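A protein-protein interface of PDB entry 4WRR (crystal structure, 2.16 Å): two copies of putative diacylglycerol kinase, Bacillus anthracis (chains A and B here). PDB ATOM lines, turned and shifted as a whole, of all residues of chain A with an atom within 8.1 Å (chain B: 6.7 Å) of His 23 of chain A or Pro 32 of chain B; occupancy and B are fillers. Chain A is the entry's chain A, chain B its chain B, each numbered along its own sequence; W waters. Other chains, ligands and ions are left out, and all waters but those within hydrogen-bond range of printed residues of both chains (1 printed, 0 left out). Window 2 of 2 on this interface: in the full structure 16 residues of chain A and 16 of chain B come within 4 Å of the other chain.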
ATOM      1  N   PRO A  15     -25.029 -21.349  -0.849  1.00  0.00           N
ATOM      2  CA  PRO A  15     -26.253 -22.039  -1.236  1.00  0.00           C
ATOM      3  C   PRO A  15     -27.452 -21.756  -0.335  1.00  0.00           C
ATOM      4  O   PRO A  15     -28.568 -22.024  -0.737  1.00  0.00           O
ATOM      5  CB  PRO A  15     -25.882 -23.523  -1.184  1.00  0.00           C
ATOM      6  CG  PRO A  15     -24.528 -23.617  -0.625  1.00  0.00           C
ATOM      7  CD  PRO A  15     -24.016 -22.257  -0.302  1.00  0.00           C
ATOM      8  N   GLY A  20     -32.484 -19.899   0.482  1.00  0.00           N
ATOM      9  CA  GLY A  20     -32.084 -21.300   0.247  1.00  0.00           C
ATOM     10  C   GLY A  20     -32.723 -22.084  -0.907  1.00  0.00           C
ATOM     11  O   GLY A  20     -32.444 -23.289  -1.035  1.00  0.00           O
ATOM     12  N   ASP A  21     -33.596 -21.458  -1.726  1.00  0.00           N
ATOM     13  CA  ASP A  21     -34.167 -22.113  -2.950  1.00  0.00           C
ATOM     14  C   ASP A  21     -33.104 -22.190  -4.093  1.00  0.00           C
ATOM     15  O   ASP A  21     -33.148 -21.448  -5.064  1.00  0.00           O
ATOM     16  CB  ASP A  21     -35.435 -21.364  -3.402  1.00  0.00           C
ATOM     17  N   LEU A  22     -32.141 -23.092  -3.940  1.00  0.00           N
ATOM     18  CA  LEU A  22     -30.875 -23.023  -4.674  1.00  0.00           C
ATOM     19  C   LEU A  22     -31.059 -23.094  -6.178  1.00  0.00           C
ATOM     20  O   LEU A  22     -30.558 -22.264  -6.919  1.00  0.00           O
ATOM     21  CB  LEU A  22     -29.931 -24.148  -4.205  1.00  0.00           C
ATOM     22  CG  LEU A  22     -28.588 -24.343  -4.948  1.00  0.00           C
ATOM     23  CD1 LEU A  22     -27.754 -23.083  -4.915  1.00  0.00           C
ATOM     24  CD2 LEU A  22     -27.806 -25.536  -4.394  1.00  0.00           C
ATOM     25  N   HIS A  23     -31.801 -24.078  -6.641  1.00  0.00           N
ATOM     26  CA  HIS A  23     -31.997 -24.294  -8.081  1.00  0.00           C
ATOM     27  C   HIS A  23     -32.680 -23.092  -8.715  1.00  0.00           C
ATOM     28  O   HIS A  23     -32.232 -22.572  -9.754  1.00  0.00           O
ATOM     29  CB  HIS A  23     -32.802 -25.608  -8.337  1.00  0.00           C
ATOM     30  CG  HIS A  23     -32.798 -26.073  -9.765  1.00  0.00           C
ATOM     31  ND1 HIS A  23     -32.627 -27.393 -10.097  1.00  0.00           N
ATOM     32  CD2 HIS A  23     -32.904 -25.408 -10.943  1.00  0.00           C
ATOM     33  CE1 HIS A  23     -32.651 -27.530 -11.410  1.00  0.00           C
ATOM     34  NE2 HIS A  23     -32.809 -26.340 -11.949  1.00  0.00           N
ATOM     35  N   THR A  24     -33.741 -22.640  -8.082  1.00  0.00           N
ATOM     36  CA  THR A  24     -34.459 -21.469  -8.562  1.00  0.00           C
ATOM     37  C   THR A  24     -33.592 -20.199  -8.559  1.00  0.00           C
ATOM     38  O   THR A  24     -33.601 -19.453  -9.531  1.00  0.00           O
ATOM     39  CB  THR A  24     -35.725 -21.234  -7.729  1.00  0.00           C
ATOM     40  OG1 THR A  24     -36.584 -22.395  -7.870  1.00  0.00           O
ATOM     41  CG2 THR A  24     -36.447 -20.046  -8.239  1.00  0.00           C
ATOM     42  N   ASN A  25     -32.813 -19.986  -7.513  1.00  0.00           N
ATOM     43  CA  ASN A  25     -31.875 -18.857  -7.509  1.00  0.00           C
ATOM     44  C   ASN A  25     -30.853 -18.953  -8.656  1.00  0.00           C
ATOM     45  O   ASN A  25     -30.534 -17.954  -9.289  1.00  0.00           O
ATOM     46  CB  ASN A  25     -31.169 -18.740  -6.153  1.00  0.00           C
ATOM     47  CG  ASN A  25     -32.129 -18.406  -5.023  1.00  0.00           C
ATOM     48  OD1 ASN A  25     -33.169 -17.805  -5.248  1.00  0.00           O
ATOM     49  ND2 ASN A  25     -31.809 -18.821  -3.820  1.00  0.00           N
ATOM     50  N   LEU A  26     -30.340 -20.160  -8.911  1.00  0.00           N
ATOM     51  CA  LEU A  26     -29.343 -20.340  -9.968  1.00  0.00           C
ATOM     52  C   LEU A  26     -29.960 -20.122 -11.350  1.00  0.00           C
ATOM     53  O   LEU A  26     -29.312 -19.643 -12.262  1.00  0.00           O
ATOM     54  CB  LEU A  26     -28.669 -21.717  -9.861  1.00  0.00           C
ATOM     55  CG  LEU A  26     -27.822 -21.908  -8.608  1.00  0.00           C
ATOM     56  CD1 LEU A  26     -27.252 -23.303  -8.459  1.00  0.00           C
ATOM     57  CD2 LEU A  26     -26.673 -20.936  -8.625  1.00  0.00           C
ATOM     58  N   THR A  27     -31.217 -20.516 -11.508  1.00  0.00           N
ATOM     59  CA  THR A  27     -31.940 -20.213 -12.740  1.00  0.00           C
ATOM     60  C   THR A  27     -31.993 -18.697 -12.989  1.00  0.00           C
ATOM     61  O   THR A  27     -31.859 -18.242 -14.118  1.00  0.00           O
ATOM     62  CB  THR A  27     -33.331 -20.836 -12.689  1.00  0.00           C
ATOM     63  OG1 THR A  27     -33.169 -22.269 -12.695  1.00  0.00           O
ATOM     64  CG2 THR A  27     -34.211 -20.381 -13.882  1.00  0.00           C
ATOM     65  N   LYS A  28     -32.153 -17.922 -11.927  1.00  0.00           N
ATOM     66  CA  LYS A  28     -32.184 -16.465 -12.051  1.00  0.00           C
ATOM     67  C   LYS A  28     -30.830 -15.807 -12.333  1.00  0.00           C
ATOM     68  O   LYS A  28     -30.754 -14.868 -13.141  1.00  0.00           O
ATOM     69  CB  LYS A  28     -32.788 -15.867 -10.807  1.00  0.00           C
ATOM     70  CG  LYS A  28     -34.285 -16.118 -10.716  1.00  0.00           C
ATOM     71  CD  LYS A  28     -34.771 -15.835  -9.314  1.00  0.00           C
ATOM     72  CE  LYS A  28     -36.274 -16.013  -9.240  1.00  0.00           C
ATOM     73  NZ  LYS A  28     -36.676 -15.724  -7.833  1.00  0.00           N
ATOM     74  N   ILE A  29     -29.758 -16.313 -11.725  1.00  0.00           N
ATOM     75  CA  ILE A  29     -28.489 -15.608 -11.786  1.00  0.00           C
ATOM     76  C   ILE A  29     -27.441 -16.166 -12.741  1.00  0.00           C
ATOM     77  O   ILE A  29     -26.657 -15.393 -13.273  1.00  0.00           O
ATOM     78  CB  ILE A  29     -27.852 -15.397 -10.392  1.00  0.00           C
ATOM     79  CG1 ILE A  29     -27.323 -16.687  -9.804  1.00  0.00           C
ATOM     80  CG2 ILE A  29     -28.840 -14.781  -9.427  1.00  0.00           C
ATOM     81  CD1 ILE A  29     -26.626 -16.471  -8.470  1.00  0.00           C
ATOM     82  N   VAL A  30     -27.419 -17.481 -12.968  1.00  0.00           N
ATOM     83  CA  VAL A  30     -26.302 -18.050 -13.711  1.00  0.00           C
ATOM     84  C   VAL A  30     -26.434 -17.826 -15.228  1.00  0.00           C
ATOM     85  O   VAL A  30     -25.479 -17.431 -15.869  1.00  0.00           O
ATOM     86  CB  VAL A  30     -26.087 -19.537 -13.362  1.00  0.00           C
ATOM     87  CG1 VAL A  30     -24.897 -20.073 -14.147  1.00  0.00           C
ATOM     88  CG2 VAL A  30     -25.825 -19.730 -11.885  1.00  0.00           C
ATOM     89  N   PRO A  31     -27.620 -18.045 -15.813  1.00  0.00           N
ATOM     90  CA  PRO A  31     -27.706 -17.876 -17.269  1.00  0.00           C
ATOM     91  C   PRO A  31     -27.289 -16.543 -17.852  1.00  0.00           C
ATOM     92  O   PRO A  31     -26.579 -16.528 -18.834  1.00  0.00           O
ATOM     93  CB  PRO A  31     -29.182 -18.160 -17.562  1.00  0.00           C
ATOM     94  CG  PRO A  31     -29.546 -19.152 -16.527  1.00  0.00           C
ATOM     95  CD  PRO A  31     -28.827 -18.717 -15.287  1.00  0.00           C
ATOM     96  N   HIS A  44     -19.578 -23.244  -4.830  1.00  0.00           N
ATOM     97  CA  HIS A  44     -20.455 -23.069  -3.684  1.00  0.00           C
ATOM     98  C   HIS A  44     -19.623 -23.063  -2.404  1.00  0.00           C
ATOM     99  O   HIS A  44     -18.687 -23.868  -2.248  1.00  0.00           O
ATOM    100  CB  HIS A  44     -21.443 -24.206  -3.567  1.00  0.00           C
ATOM    101  CG  HIS A  44     -22.286 -24.420  -4.782  1.00  0.00           C
ATOM    102  ND1 HIS A  44     -23.368 -25.274  -4.777  1.00  0.00           N
ATOM    103  CD2 HIS A  44     -22.184 -23.952  -6.042  1.00  0.00           C
ATOM    104  CE1 HIS A  44     -23.922 -25.288  -5.973  1.00  0.00           C
ATOM    105  NE2 HIS A  44     -23.254 -24.451  -6.744  1.00  0.00           N
ATOM    106  N   LEU B  26     -28.662 -21.892 -22.132  1.00  0.00           N
ATOM    107  CA  LEU B  26     -27.986 -21.898 -20.826  1.00  0.00           C
ATOM    108  C   LEU B  26     -28.963 -21.939 -19.678  1.00  0.00           C
ATOM    109  O   LEU B  26     -28.709 -22.543 -18.654  1.00  0.00           O
ATOM    110  CB  LEU B  26     -27.038 -20.720 -20.712  1.00  0.00           C
ATOM    111  CG  LEU B  26     -25.855 -20.762 -21.696  1.00  0.00           C
ATOM    112  CD1 LEU B  26     -24.991 -19.494 -21.637  1.00  0.00           C
ATOM    113  CD2 LEU B  26     -24.979 -21.925 -21.395  1.00  0.00           C
ATOM    114  N   THR B  27     -30.108 -21.312 -19.864  1.00  0.00           N
ATOM    115  CA  THR B  27     -31.188 -21.418 -18.879  1.00  0.00           C
ATOM    116  C   THR B  27     -31.606 -22.881 -18.699  1.00  0.00           C
ATOM    117  O   THR B  27     -31.896 -23.323 -17.598  1.00  0.00           O
ATOM    118  CB  THR B  27     -32.347 -20.529 -19.306  1.00  0.00           C
ATOM    119  OG1 THR B  27     -31.894 -19.167 -19.242  1.00  0.00           O
ATOM    120  CG2 THR B  27     -33.577 -20.728 -18.414  1.00  0.00           C
ATOM    121  N   LYS B  28     -31.619 -23.639 -19.788  1.00  0.00           N
ATOM    122  CA  LYS B  28     -32.016 -25.042 -19.718  1.00  0.00           C
ATOM    123  C   LYS B  28     -30.960 -25.964 -19.111  1.00  0.00           C
ATOM    124  O   LYS B  28     -31.304 -26.879 -18.351  1.00  0.00           O
ATOM    125  CB  LYS B  28     -32.368 -25.544 -21.107  1.00  0.00           C
ATOM    126  CG  LYS B  28     -33.708 -25.011 -21.604  1.00  0.00           C
ATOM    127  CD  LYS B  28     -33.847 -25.207 -23.083  1.00  0.00           C
ATOM    128  CE  LYS B  28     -35.190 -24.723 -23.592  1.00  0.00           C
ATOM    129  NZ  LYS B  28     -35.245 -24.971 -25.062  1.00  0.00           N
ATOM    130  N   ILE B  29     -29.683 -25.716 -19.388  1.00  0.00           N
ATOM    131  CA  ILE B  29     -28.664 -26.690 -19.006  1.00  0.00           C
ATOM    132  C   ILE B  29     -27.828 -26.341 -17.809  1.00  0.00           C
ATOM    133  O   ILE B  29     -27.392 -27.246 -17.108  1.00  0.00           O
ATOM    134  CB  ILE B  29     -27.723 -27.049 -20.167  1.00  0.00           C
ATOM    135  CG1 ILE B  29     -26.785 -25.906 -20.549  1.00  0.00           C
ATOM    136  CG2 ILE B  29     -28.519 -27.470 -21.390  1.00  0.00           C
ATOM    137  CD1 ILE B  29     -25.791 -26.315 -21.639  1.00  0.00           C
ATOM    138  N   VAL B  30     -27.613 -25.056 -17.525  1.00  0.00           N
ATOM    139  CA  VAL B  30     -26.660 -24.731 -16.498  1.00  0.00           C
ATOM    140  C   VAL B  30     -27.237 -24.908 -15.080  1.00  0.00           C
ATOM    141  O   VAL B  30     -26.569 -25.443 -14.209  1.00  0.00           O
ATOM    142  CB  VAL B  30     -26.041 -23.327 -16.718  1.00  0.00           C
ATOM    143  CG1 VAL B  30     -25.006 -23.027 -15.634  1.00  0.00           C
ATOM    144  CG2 VAL B  30     -25.338 -23.228 -18.071  1.00  0.00           C
ATOM    145  N   PRO B  31     -28.457 -24.413 -14.815  1.00  0.00           N
ATOM    146  CA  PRO B  31     -28.934 -24.475 -13.432  1.00  0.00           C
ATOM    147  C   PRO B  31     -28.972 -25.874 -12.807  1.00  0.00           C
ATOM    148  O   PRO B  31     -28.599 -26.001 -11.670  1.00  0.00           O
ATOM    149  CB  PRO B  31     -30.346 -23.877 -13.544  1.00  0.00           C
ATOM    150  CG  PRO B  31     -30.205 -22.866 -14.613  1.00  0.00           C
ATOM    151  CD  PRO B  31     -29.289 -23.499 -15.628  1.00  0.00           C
ATOM    152  N   PRO B  32     -29.451 -26.915 -13.520  1.00  0.00           N
ATOM    153  CA  PRO B  32     -29.347 -28.254 -12.923  1.00  0.00           C
ATOM    154  C   PRO B  32     -27.919 -28.658 -12.579  1.00  0.00           C
ATOM    155  O   PRO B  32     -27.676 -29.288 -11.574  1.00  0.00           O
ATOM    156  CB  PRO B  32     -29.902 -29.186 -14.018  1.00  0.00           C
ATOM    157  CG  PRO B  32     -30.611 -28.314 -14.984  1.00  0.00           C
ATOM    158  CD  PRO B  32     -29.957 -26.980 -14.902  1.00  0.00           C
ATOM    159  N   LEU B  33     -26.981 -28.311 -13.440  1.00  0.00           N
ATOM    160  CA  LEU B  33     -25.583 -28.695 -13.249  1.00  0.00           C
ATOM    161  C   LEU B  33     -24.953 -27.902 -12.120  1.00  0.00           C
ATOM    162  O   LEU B  33     -24.324 -28.472 -11.235  1.00  0.00           O
ATOM    163  CB  LEU B  33     -24.822 -28.465 -14.540  1.00  0.00           C
ATOM    164  CG  LEU B  33     -25.219 -29.306 -15.742  1.00  0.00           C
ATOM    165  CD1 LEU B  33     -24.446 -28.922 -16.981  1.00  0.00           C
ATOM    166  CD2 LEU B  33     -25.033 -30.792 -15.459  1.00  0.00           C
ATOM    167  N   ALA B  34     -25.173 -26.585 -12.118  1.00  0.00           N
ATOM    168  CA  ALA B  34     -24.689 -25.737 -11.047  1.00  0.00           C
ATOM    169  C   ALA B  34     -25.308 -26.049  -9.700  1.00  0.00           C
ATOM    170  O   ALA B  34     -24.634 -25.895  -8.697  1.00  0.00           O
ATOM    171  CB  ALA B  34     -24.890 -24.274 -11.367  1.00  0.00           C
ATOM    172  N   ALA B  35     -26.561 -26.512  -9.644  1.00  0.00           N
ATOM    173  CA  ALA B  35     -27.145 -26.926  -8.349  1.00  0.00           C
ATOM    174  C   ALA B  35     -26.516 -28.187  -7.842  1.00  0.00           C
ATOM    175  O   ALA B  35     -26.274 -28.334  -6.648  1.00  0.00           O
ATOM    176  CB  ALA B  35     -28.643 -27.124  -8.453  1.00  0.00           C
ATOM    177  N   ALA B  36     -26.237 -29.115  -8.756  1.00  0.00           N
ATOM    178  CA  ALA B  36     -25.724 -30.443  -8.373  1.00  0.00           C
ATOM    179  C   ALA B  36     -24.211 -30.495  -8.153  1.00  0.00           C
ATOM    180  O   ALA B  36     -23.743 -31.306  -7.376  1.00  0.00           O
ATOM    181  CB  ALA B  36     -26.104 -31.459  -9.416  1.00  0.00           C
ATOM    182  N   PHE B  37     -23.446 -29.635  -8.841  1.00  0.00           N
ATOM    183  CA  PHE B  37     -21.979 -29.725  -8.854  1.00  0.00           C
ATOM    184  C   PHE B  37     -21.430 -28.413  -8.282  1.00  0.00           C
ATOM    185  O   PHE B  37     -21.420 -27.406  -8.955  1.00  0.00           O
ATOM    186  CB  PHE B  37     -21.464 -29.964 -10.273  1.00  0.00           C
ATOM    187  CG  PHE B  37     -21.920 -31.271 -10.878  1.00  0.00           C
ATOM    188  CD1 PHE B  37     -21.597 -32.477 -10.279  1.00  0.00           C
ATOM    189  CD2 PHE B  37     -22.684 -31.291 -12.028  1.00  0.00           C
ATOM    190  CE1 PHE B  37     -22.025 -33.672 -10.807  1.00  0.00           C
ATOM    191  CE2 PHE B  37     -23.101 -32.488 -12.583  1.00  0.00           C
ATOM    192  CZ  PHE B  37     -22.783 -33.685 -11.971  1.00  0.00           C
ATOM    193  N   ALA B 112     -32.486 -29.880 -21.496  1.00  0.00           N
ATOM    194  CA  ALA B 112     -32.689 -29.799 -20.050  1.00  0.00           C
ATOM    195  C   ALA B 112     -32.673 -31.180 -19.417  1.00  0.00           C
ATOM    196  O   ALA B 112     -32.107 -31.376 -18.333  1.00  0.00           O
ATOM    197  CB  ALA B 112     -33.988 -29.068 -19.704  1.00  0.00           C
ATOM    198  N   ALA B 115     -29.172 -32.591 -19.270  1.00  0.00           N
ATOM    199  CA  ALA B 115     -28.405 -32.009 -18.177  1.00  0.00           C
ATOM    200  C   ALA B 115     -28.753 -32.648 -16.831  1.00  0.00           C
ATOM    201  O   ALA B 115     -27.849 -33.000 -16.053  1.00  0.00           O
ATOM    202  CB  ALA B 115     -28.641 -30.503 -18.128  1.00  0.00           C
ATOM    203  N   LYS B 116     -30.046 -32.818 -16.558  1.00  0.00           N
ATOM    204  CA  LYS B 116     -30.504 -33.522 -15.350  1.00  0.00           C
ATOM    205  C   LYS B 116     -29.924 -34.919 -15.255  1.00  0.00           C
ATOM    206  O   LYS B 116     -29.565 -35.370 -14.176  1.00  0.00           O
ATOM    207  CB  LYS B 116     -32.047 -33.600 -15.245  1.00  0.00           C
ATOM    208  N   THR B 119     -26.635 -35.284 -13.635  1.00  0.00           N
ATOM    209  CA  THR B 119     -26.661 -35.164 -12.176  1.00  0.00           C
ATOM    210  C   THR B 119     -26.932 -36.498 -11.486  1.00  0.00           C
ATOM    211  O   THR B 119     -26.647 -36.646 -10.291  1.00  0.00           O
ATOM    212  CB  THR B 119     -27.671 -34.101 -11.659  1.00  0.00           C
ATOM    213  OG1 THR B 119     -28.995 -34.546 -11.845  1.00  0.00           O
ATOM    214  CG2 THR B 119     -27.502 -32.784 -12.367  1.00  0.00           C
HETATM  215  O   HOH W   1     -21.284 -24.621  -9.248  1.00  0.00           O
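Thr 27 of chain A touches Pro 31 of chain B, and with the chains exchanged Pro 31 of chain A touches Thr 27 of chain B. Val 30 of chain B touches its own counterpart, Val 30 of chain A. Positions printed for both chains: 26, 27, 28, 29, 30 and 31.
Leu 22 of chain A touches Ala 35 of chain B (CD2 to O, 3.9 Å). His 23 of chain A touches Pro 31 of chain B. CA of Pro 32 of chain B touches CE1 of His 23 of chain A, 3.7 Å away. CD1 of Leu 26 of chain A touches C of Ala 34 of chain B, 3.6 Å away. Leu 26 of chain A touches Ala 35 of chain B (CD1 to N, 3.5 Å). CB of Pro 31 of chain B touches OG1 of Thr 27 of chain A (3.4 Å). Val 30 of chain B touches Val 30 of chain A. Pro 31 of chain A touches Thr 27 of chain B. His 44 of chain A touches Ala 35 of chain B (CE1 to O, 3.9 Å).
O of His 23 of chain A lies within hydrogen-bond range of OG1 of Thr 27 of chain A, at 3.1 Å.
Of the printed residues of chain B, His 23 of chain A touches Pro 31 and Pro 32. Of the printed residues of chain A, Pro 31 of chain B touches His 23 (3.8 Å) and Thr 27 (3.4 Å). Printed residues of chain B within 4 Å of His 44 of chain A: Ala 34 and Ala 35. Gly 20 of chain A touches none of the printed residues of chain B. The nearest residue of chain A that does not touch Pro 32 of chain B is Thr 27 of chain A (6.0 Å). The nearest printed residue of chain B that does not touch His 44 of chain A is Phe 37 of chain B (4.1 Å).
Printed residues of chain B that touch a printed residue of chain A: Thr 27, Val 30, Pro 31, Pro 32, Ala 34 and Ala 35. Hydrophobic or aromatic side chains of chain B within 4 Å of the printed part of chain A: Val 30, Pro 31 and Ala 34.
Water W1 bridges the backbone carbonyl oxygen of Phe 37 of chain B (2.8 Å) and a ring nitrogen (NE2) of His 44 of chain A (3.2 Å).
A ring nitrogen (NE2) of His 44 of chain A is in hydrogen-bond range of the backbone carbonyl oxygen of Ala 34 of chain B, at 2.8 Å.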
